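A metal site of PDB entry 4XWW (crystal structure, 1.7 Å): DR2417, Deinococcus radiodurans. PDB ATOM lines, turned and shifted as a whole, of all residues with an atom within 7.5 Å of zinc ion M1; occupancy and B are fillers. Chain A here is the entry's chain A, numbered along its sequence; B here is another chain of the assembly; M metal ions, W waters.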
ATOM      1  N   ILE A  30     -13.112   9.166 -32.824  1.00  0.00           N
ATOM      2  CA  ILE A  30     -13.765  10.342 -32.302  1.00  0.00           C
ATOM      3  C   ILE A  30     -14.512   9.911 -31.031  1.00  0.00           C
ATOM      4  O   ILE A  30     -15.547   9.247 -31.102  1.00  0.00           O
ATOM      5  CB  ILE A  30     -14.702  10.958 -33.317  1.00  0.00           C
ATOM      6  CG1 ILE A  30     -13.884  11.409 -34.537  1.00  0.00           C
ATOM      7  CG2 ILE A  30     -15.471  12.122 -32.686  1.00  0.00           C
ATOM      8  CD1 ILE A  30     -14.679  12.045 -35.629  1.00  0.00           C
ATOM      9  N   GLY A  31     -13.967  10.292 -29.876  1.00  0.00           N
ATOM     10  CA  GLY A  31     -14.511   9.879 -28.595  1.00  0.00           C
ATOM     11  C   GLY A  31     -13.459   9.543 -27.549  1.00  0.00           C
ATOM     12  O   GLY A  31     -12.267   9.347 -27.873  1.00  0.00           O
ATOM     13  N   LYS A  32     -13.925   9.463 -26.308  1.00  0.00           N
ATOM     14  CA  LYS A  32     -13.149   9.220 -25.085  1.00  0.00           C
ATOM     15  C   LYS A  32     -11.756   9.825 -25.088  1.00  0.00           C
ATOM     16  O   LYS A  32     -10.754   9.145 -24.844  1.00  0.00           O
ATOM     17  CB  LYS A  32     -13.072   7.707 -24.749  1.00  0.00           C
ATOM     18  CG  LYS A  32     -12.465   6.768 -25.801  1.00  0.00           C
ATOM     19  CD  LYS A  32     -12.608   5.302 -25.303  1.00  0.00           C
ATOM     20  CE  LYS A  32     -12.270   4.259 -26.387  1.00  0.00           C
ATOM     21  NZ  LYS A  32     -10.837   4.366 -26.805  1.00  0.00           N
ATOM     22  N   ASN A  33     -11.702  11.133 -25.318  1.00  0.00           N
ATOM     23  CA  ASN A  33     -10.454  11.865 -25.335  1.00  0.00           C
ATOM     24  C   ASN A  33      -9.775  11.878 -23.972  1.00  0.00           C
ATOM     25  O   ASN A  33     -10.408  12.173 -22.951  1.00  0.00           O
ATOM     26  CB  ASN A  33     -10.725  13.280 -25.824  1.00  0.00           C
ATOM     27  CG  ASN A  33     -11.172  13.295 -27.272  1.00  0.00           C
ATOM     28  OD1 ASN A  33     -10.350  13.124 -28.155  1.00  0.00           O
ATOM     29  ND2 ASN A  33     -12.456  13.457 -27.517  1.00  0.00           N
ATOM     30  N   ASP A  47      -8.313  15.990 -19.990  1.00  0.00           N
ATOM     31  CA  ASP A  47      -9.641  15.490 -20.326  1.00  0.00           C
ATOM     32  C   ASP A  47      -9.839  14.055 -19.830  1.00  0.00           C
ATOM     33  O   ASP A  47      -8.884  13.372 -19.485  1.00  0.00           O
ATOM     34  CB  ASP A  47      -9.927  15.654 -21.817  1.00  0.00           C
ATOM     35  CG  ASP A  47     -10.235  17.085 -22.198  1.00  0.00           C
ATOM     36  OD1 ASP A  47     -10.435  17.910 -21.279  1.00  0.00           O
ATOM     37  OD2 ASP A  47     -10.270  17.406 -23.405  1.00  0.00           O
ATOM     38  N   THR A  83     -10.832  20.749 -21.025  1.00  0.00           N
ATOM     39  CA  THR A  83     -10.946  21.766 -22.075  1.00  0.00           C
ATOM     40  C   THR A  83     -12.375  22.276 -22.300  1.00  0.00           C
ATOM     41  O   THR A  83     -12.571  23.431 -22.650  1.00  0.00           O
ATOM     42  CB  THR A  83     -10.383  21.279 -23.440  1.00  0.00           C
ATOM     43  OG1 THR A  83     -11.103  20.127 -23.899  1.00  0.00           O
ATOM     44  CG2 THR A  83      -8.877  20.945 -23.336  1.00  0.00           C
ATOM     45  N   HIS A  84     -13.363  21.402 -22.110  1.00  0.00           N
ATOM     46  CA  HIS A  84     -14.773  21.767 -22.270  1.00  0.00           C
ATOM     47  C   HIS A  84     -15.668  20.616 -21.800  1.00  0.00           C
ATOM     48  O   HIS A  84     -15.186  19.507 -21.568  1.00  0.00           O
ATOM     49  CB  HIS A  84     -15.133  22.164 -23.729  1.00  0.00           C
ATOM     50  CG  HIS A  84     -15.012  21.063 -24.745  1.00  0.00           C
ATOM     51  ND1 HIS A  84     -13.818  20.482 -25.096  1.00  0.00           N
ATOM     52  CD2 HIS A  84     -15.952  20.507 -25.577  1.00  0.00           C
ATOM     53  CE1 HIS A  84     -14.011  19.601 -26.072  1.00  0.00           C
ATOM     54  NE2 HIS A  84     -15.297  19.613 -26.374  1.00  0.00           N
ATOM     55  N   HIS A  86     -18.153  18.776 -23.125  1.00  0.00           N
ATOM     56  CA  HIS A  86     -18.750  17.705 -23.957  1.00  0.00           C
ATOM     57  C   HIS A  86     -18.471  16.333 -23.365  1.00  0.00           C
ATOM     58  O   HIS A  86     -17.435  16.099 -22.757  1.00  0.00           O
ATOM     59  CB  HIS A  86     -18.208  17.752 -25.402  1.00  0.00           C
ATOM     60  CG  HIS A  86     -18.947  18.690 -26.291  1.00  0.00           C
ATOM     61  ND1 HIS A  86     -18.349  19.334 -27.357  1.00  0.00           N
ATOM     62  CD2 HIS A  86     -20.235  19.120 -26.270  1.00  0.00           C
ATOM     63  CE1 HIS A  86     -19.236  20.113 -27.954  1.00  0.00           C
ATOM     64  NE2 HIS A  86     -20.390  19.992 -27.329  1.00  0.00           N
ATOM     65  N   GLU A  87     -19.402  15.394 -23.566  1.00  0.00           N
ATOM     66  CA  GLU A  87     -19.285  14.063 -22.998  1.00  0.00           C
ATOM     67  C   GLU A  87     -18.069  13.297 -23.494  1.00  0.00           C
ATOM     68  O   GLU A  87     -17.567  12.468 -22.769  1.00  0.00           O
ATOM     69  CB  GLU A  87     -20.547  13.244 -23.284  1.00  0.00           C
ATOM     70  CG  GLU A  87     -21.748  13.668 -22.426  1.00  0.00           C
ATOM     71  CD  GLU A  87     -21.660  13.230 -20.987  1.00  0.00           C
ATOM     72  OE1 GLU A  87     -20.764  12.448 -20.630  1.00  0.00           O
ATOM     73  OE2 GLU A  87     -22.514  13.677 -20.199  1.00  0.00           O
ATOM     74  N   ASP A  88     -17.591  13.571 -24.702  1.00  0.00           N
ATOM     75  CA  ASP A  88     -16.388  12.852 -25.126  1.00  0.00           C
ATOM     76  C   ASP A  88     -15.112  13.499 -24.586  1.00  0.00           C
ATOM     77  O   ASP A  88     -14.001  13.086 -24.952  1.00  0.00           O
ATOM     78  CB  ASP A  88     -16.316  12.739 -26.658  1.00  0.00           C
ATOM     79  CG  ASP A  88     -16.090  14.059 -27.339  1.00  0.00           C
ATOM     80  OD1 ASP A  88     -16.745  15.051 -26.932  1.00  0.00           O
ATOM     81  OD2 ASP A  88     -15.281  14.099 -28.283  1.00  0.00           O
ATOM     82  N   HIS A  89     -15.257  14.472 -23.684  1.00  0.00           N
ATOM     83  CA  HIS A  89     -14.113  14.992 -22.941  1.00  0.00           C
ATOM     84  C   HIS A  89     -14.267  14.894 -21.427  1.00  0.00           C
ATOM     85  O   HIS A  89     -13.256  14.880 -20.727  1.00  0.00           O
ATOM     86  CB  HIS A  89     -13.819  16.433 -23.365  1.00  0.00           C
ATOM     87  CG  HIS A  89     -13.504  16.550 -24.828  1.00  0.00           C
ATOM     88  ND1 HIS A  89     -12.211  16.715 -25.295  1.00  0.00           N
ATOM     89  CD2 HIS A  89     -14.290  16.471 -25.923  1.00  0.00           C
ATOM     90  CE1 HIS A  89     -12.230  16.758 -26.618  1.00  0.00           C
ATOM     91  NE2 HIS A  89     -13.480  16.615 -27.026  1.00  0.00           N
ATOM     92  N   HIS A 153     -16.559  26.871 -30.275  1.00  0.00           N
ATOM     93  CA  HIS A 153     -16.957  25.469 -30.411  1.00  0.00           C
ATOM     94  C   HIS A 153     -18.476  25.455 -30.228  1.00  0.00           C
ATOM     95  O   HIS A 153     -19.101  26.512 -30.150  1.00  0.00           O
ATOM     96  CB  HIS A 153     -16.205  24.623 -29.361  1.00  0.00           C
ATOM     97  CG  HIS A 153     -16.306  23.134 -29.553  1.00  0.00           C
ATOM     98  ND1 HIS A 153     -16.493  22.541 -30.796  1.00  0.00           N
ATOM     99  CD2 HIS A 153     -16.264  22.121 -28.654  1.00  0.00           C
ATOM    100  CE1 HIS A 153     -16.549  21.230 -30.632  1.00  0.00           C
ATOM    101  NE2 HIS A 153     -16.436  20.956 -29.354  1.00  0.00           N
ATOM    102  N   GLY A 174      -7.621  22.289 -28.696  1.00  0.00           N
ATOM    103  CA  GLY A 174      -8.874  21.728 -28.231  1.00  0.00           C
ATOM    104  C   GLY A 174      -9.759  21.405 -29.421  1.00  0.00           C
ATOM    105  O   GLY A 174      -9.325  21.446 -30.572  1.00  0.00           O
ATOM    106  N   ASP A 175     -11.000  21.068 -29.125  1.00  0.00           N
ATOM    107  CA  ASP A 175     -12.013  20.945 -30.169  1.00  0.00           C
ATOM    108  C   ASP A 175     -12.441  22.351 -30.538  1.00  0.00           C
ATOM    109  O   ASP A 175     -12.708  23.168 -29.641  1.00  0.00           O
ATOM    110  CB  ASP A 175     -13.188  20.099 -29.659  1.00  0.00           C
ATOM    111  N   ASP A 209      -7.556  19.581 -33.940  1.00  0.00           N
ATOM    112  CA  ASP A 209      -8.818  18.870 -34.124  1.00  0.00           C
ATOM    113  C   ASP A 209      -9.042  18.472 -35.580  1.00  0.00           C
ATOM    114  O   ASP A 209      -9.183  19.323 -36.439  1.00  0.00           O
ATOM    115  CB  ASP A 209      -9.929  19.807 -33.624  1.00  0.00           C
ATOM    116  CG  ASP A 209     -11.332  19.240 -33.767  1.00  0.00           C
ATOM    117  OD1 ASP A 209     -11.526  18.071 -34.187  1.00  0.00           O
ATOM    118  OD2 ASP A 209     -12.267  20.001 -33.404  1.00  0.00           O
ATOM    119  N   THR A 211     -11.552  16.538 -36.864  1.00  0.00           N
ATOM    120  CA  THR A 211     -12.906  16.043 -37.117  1.00  0.00           C
ATOM    121  C   THR A 211     -13.396  16.292 -38.540  1.00  0.00           C
ATOM    122  O   THR A 211     -13.893  15.368 -39.222  1.00  0.00           O
ATOM    123  CB  THR A 211     -13.904  16.702 -36.142  1.00  0.00           C
ATOM    124  OG1 THR A 211     -13.504  16.413 -34.800  1.00  0.00           O
ATOM    125  CG2 THR A 211     -15.302  16.139 -36.374  1.00  0.00           C
ATOM    126  N   HIS A 381     -17.080  21.938 -35.440  1.00  0.00           N
ATOM    127  CA  HIS A 381     -15.652  21.737 -35.729  1.00  0.00           C
ATOM    128  C   HIS A 381     -15.203  22.410 -37.041  1.00  0.00           C
ATOM    129  O   HIS A 381     -15.928  22.475 -38.029  1.00  0.00           O
ATOM    130  CB  HIS A 381     -15.308  20.244 -35.770  1.00  0.00           C
ATOM    131  CG  HIS A 381     -15.648  19.496 -34.515  1.00  0.00           C
ATOM    132  ND1 HIS A 381     -14.726  19.290 -33.508  1.00  0.00           N
ATOM    133  CD2 HIS A 381     -16.801  18.918 -34.101  1.00  0.00           C
ATOM    134  CE1 HIS A 381     -15.288  18.590 -32.536  1.00  0.00           C
ATOM    135  NE2 HIS A 381     -16.542  18.351 -32.871  1.00  0.00           N
ATOM    136  N   TRP A 402      -5.276  15.106 -34.401  1.00  0.00           N
ATOM    137  CA  TRP A 402      -5.908  14.501 -33.244  1.00  0.00           C
ATOM    138  C   TRP A 402      -7.438  14.554 -33.379  1.00  0.00           C
ATOM    139  O   TRP A 402      -7.929  15.178 -34.323  1.00  0.00           O
ATOM    140  CB  TRP A 402      -5.372  15.233 -31.977  1.00  0.00           C
ATOM    141  CG  TRP A 402      -6.231  15.157 -30.766  1.00  0.00           C
ATOM    142  CD1 TRP A 402      -6.243  14.165 -29.820  1.00  0.00           C
ATOM    143  CD2 TRP A 402      -7.195  16.128 -30.343  1.00  0.00           C
ATOM    144  NE1 TRP A 402      -7.176  14.441 -28.858  1.00  0.00           N
ATOM    145  CE2 TRP A 402      -7.780  15.640 -29.161  1.00  0.00           C
ATOM    146  CE3 TRP A 402      -7.622  17.350 -30.857  1.00  0.00           C
ATOM    147  CZ2 TRP A 402      -8.771  16.347 -28.460  1.00  0.00           C
ATOM    148  CZ3 TRP A 402      -8.643  18.056 -30.179  1.00  0.00           C
ATOM    149  CH2 TRP A 402      -9.196  17.539 -28.996  1.00  0.00           C
ATOM    150  N   HIS A 403      -8.185  13.887 -32.493  1.00  0.00           N
ATOM    151  CA  HIS A 403      -9.654  13.944 -32.518  1.00  0.00           C
ATOM    152  C   HIS A 403     -10.204  13.574 -33.899  1.00  0.00           C
ATOM    153  O   HIS A 403     -10.956  14.328 -34.536  1.00  0.00           O
ATOM    154  CB  HIS A 403     -10.151  15.351 -32.082  1.00  0.00           C
ATOM    155  CG  HIS A 403     -11.572  15.386 -31.566  1.00  0.00           C
ATOM    156  ND1 HIS A 403     -12.653  15.325 -32.418  1.00  0.00           N
ATOM    157  CD2 HIS A 403     -12.078  15.540 -30.330  1.00  0.00           C
ATOM    158  CE1 HIS A 403     -13.774  15.416 -31.717  1.00  0.00           C
ATOM    159  NE2 HIS A 403     -13.453  15.538 -30.441  1.00  0.00           N
ATOM    160  P     U B   2     -21.015  18.429 -35.624  1.00  0.00           P
ATOM    161  OP1   U B   2     -21.175  19.284 -34.421  1.00  0.00           O
ATOM    162  OP2   U B   2     -19.949  18.738 -36.607  1.00  0.00           O
ATOM    163  O5'   U B   2     -20.786  16.919 -35.178  1.00  0.00           O
ATOM    164  C5'   U B   2     -21.625  16.300 -34.185  1.00  0.00           C
ATOM    165  C4'   U B   2     -20.805  15.346 -33.336  1.00  0.00           C
ATOM    166  O4'   U B   2     -20.477  14.152 -34.097  1.00  0.00           O
ATOM    167  C3'   U B   2     -19.478  15.896 -32.828  1.00  0.00           C
ATOM    168  O3'   U B   2     -19.284  15.466 -31.489  1.00  0.00           O
ATOM    169  C2'   U B   2     -18.445  15.192 -33.710  1.00  0.00           C
ATOM    170  O2'   U B   2     -17.178  15.072 -33.096  1.00  0.00           O
ATOM    171  C1'   U B   2     -19.113  13.843 -33.907  1.00  0.00           C
ATOM    172  N1    U B   2     -18.636  13.093 -35.069  1.00  0.00           N
ATOM    173  C2    U B   2     -18.420  11.734 -34.918  1.00  0.00           C
ATOM    174  O2    U B   2     -18.630  11.146 -33.875  1.00  0.00           O
ATOM    175  N3    U B   2     -17.967  11.085 -36.040  1.00  0.00           N
ATOM    176  C4    U B   2     -17.696  11.644 -37.268  1.00  0.00           C
ATOM    177  O4    U B   2     -17.292  10.931 -38.189  1.00  0.00           O
ATOM    178  C5    U B   2     -17.933  13.053 -37.344  1.00  0.00           C
ATOM    179  C6    U B   2     -18.387  13.714 -36.272  1.00  0.00           C
ATOM    180  P     U B   3     -18.677  16.467 -30.405  1.00  0.00           P
ATOM    181  OP1   U B   3     -18.472  17.771 -31.061  1.00  0.00           O
ATOM    182  OP2   U B   3     -17.537  15.781 -29.745  1.00  0.00           O
ATOM    183  O5'   U B   3     -19.868  16.633 -29.368  1.00  0.00           O
ATOM    184  C5'   U B   3     -21.163  17.039 -29.810  1.00  0.00           C
ATOM    185  C4'   U B   3     -22.220  16.220 -29.117  1.00  0.00           C
ATOM    186  O4'   U B   3     -22.445  14.989 -29.860  1.00  0.00           O
ATOM    187  C3'   U B   3     -21.885  15.815 -27.691  1.00  0.00           C
ATOM    188  O3'   U B   3     -23.020  15.979 -26.854  1.00  0.00           O
ATOM    189  C2'   U B   3     -21.516  14.340 -27.817  1.00  0.00           C
ATOM    190  O2'   U B   3     -21.766  13.583 -26.654  1.00  0.00           O
ATOM    191  C1'   U B   3     -22.423  13.900 -28.963  1.00  0.00           C
ATOM    192  N1    U B   3     -21.940  12.712 -29.673  1.00  0.00           N
ATOM    193  C2    U B   3     -22.822  11.674 -29.876  1.00  0.00           C
ATOM    194  O2    U B   3     -23.974  11.710 -29.504  1.00  0.00           O
ATOM    195  N3    U B   3     -22.292  10.586 -30.536  1.00  0.00           N
ATOM    196  C4    U B   3     -21.001  10.442 -31.001  1.00  0.00           C
ATOM    197  O4    U B   3     -20.684   9.401 -31.575  1.00  0.00           O
ATOM    198  C5    U B   3     -20.146  11.565 -30.746  1.00  0.00           C
ATOM    199  C6    U B   3     -20.632  12.635 -30.101  1.00  0.00           C
HETATM  200 ZN    ZN M   1     -14.682  16.162 -28.766  1.00  0.00          ZN
HETATM  201 ZN    ZN M   2     -16.417  19.165 -28.142  1.00  0.00          ZN
HETATM  202  O   HOH W   1     -15.747  17.815 -29.243  1.00  0.00           O
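NE2 of His 89 lies close to ND2 of Asn 33 (3.4 Å).
The side-chain carboxylate (OD2) of Asp 47 lies within hydrogen-bond range of a ring nitrogen (ND1) of His 89 (2.8 Å).
A ring nitrogen (ND1) of His 403 lies within hydrogen-bond range of the side-chain hydroxyl (OG1) of Thr 211, at 2.8 Å.
OD1 of Asp 209 sits at hydrogen-bond distance from ND1 of His 403.
The side-chain amide nitrogen of Asn 33 lies within hydrogen-bond range of the backbone carbonyl oxygen of Asp 88 (3.0 Å).
OP1 of U 3 of chain B sits at hydrogen-bond distance from a ring nitrogen (NE2) of His 381 (2.7 Å).
Merely in contact with zinc ion M1: Asn 33 (3.7 Å) and U 3 of chain B (3.0 Å).
Of the 21 residues printed, 5 come within 4 Å of zinc ion M1.
Zinc ion M1 is bound by water W1 (2.0 Å).
Zinc ion M1 is bound by NE2 of His 89.
Zinc ion M1 is bound by NE2 of His 403 (2.2 Å).
Zinc ion M1 is bound by OD2 of Asp 88.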
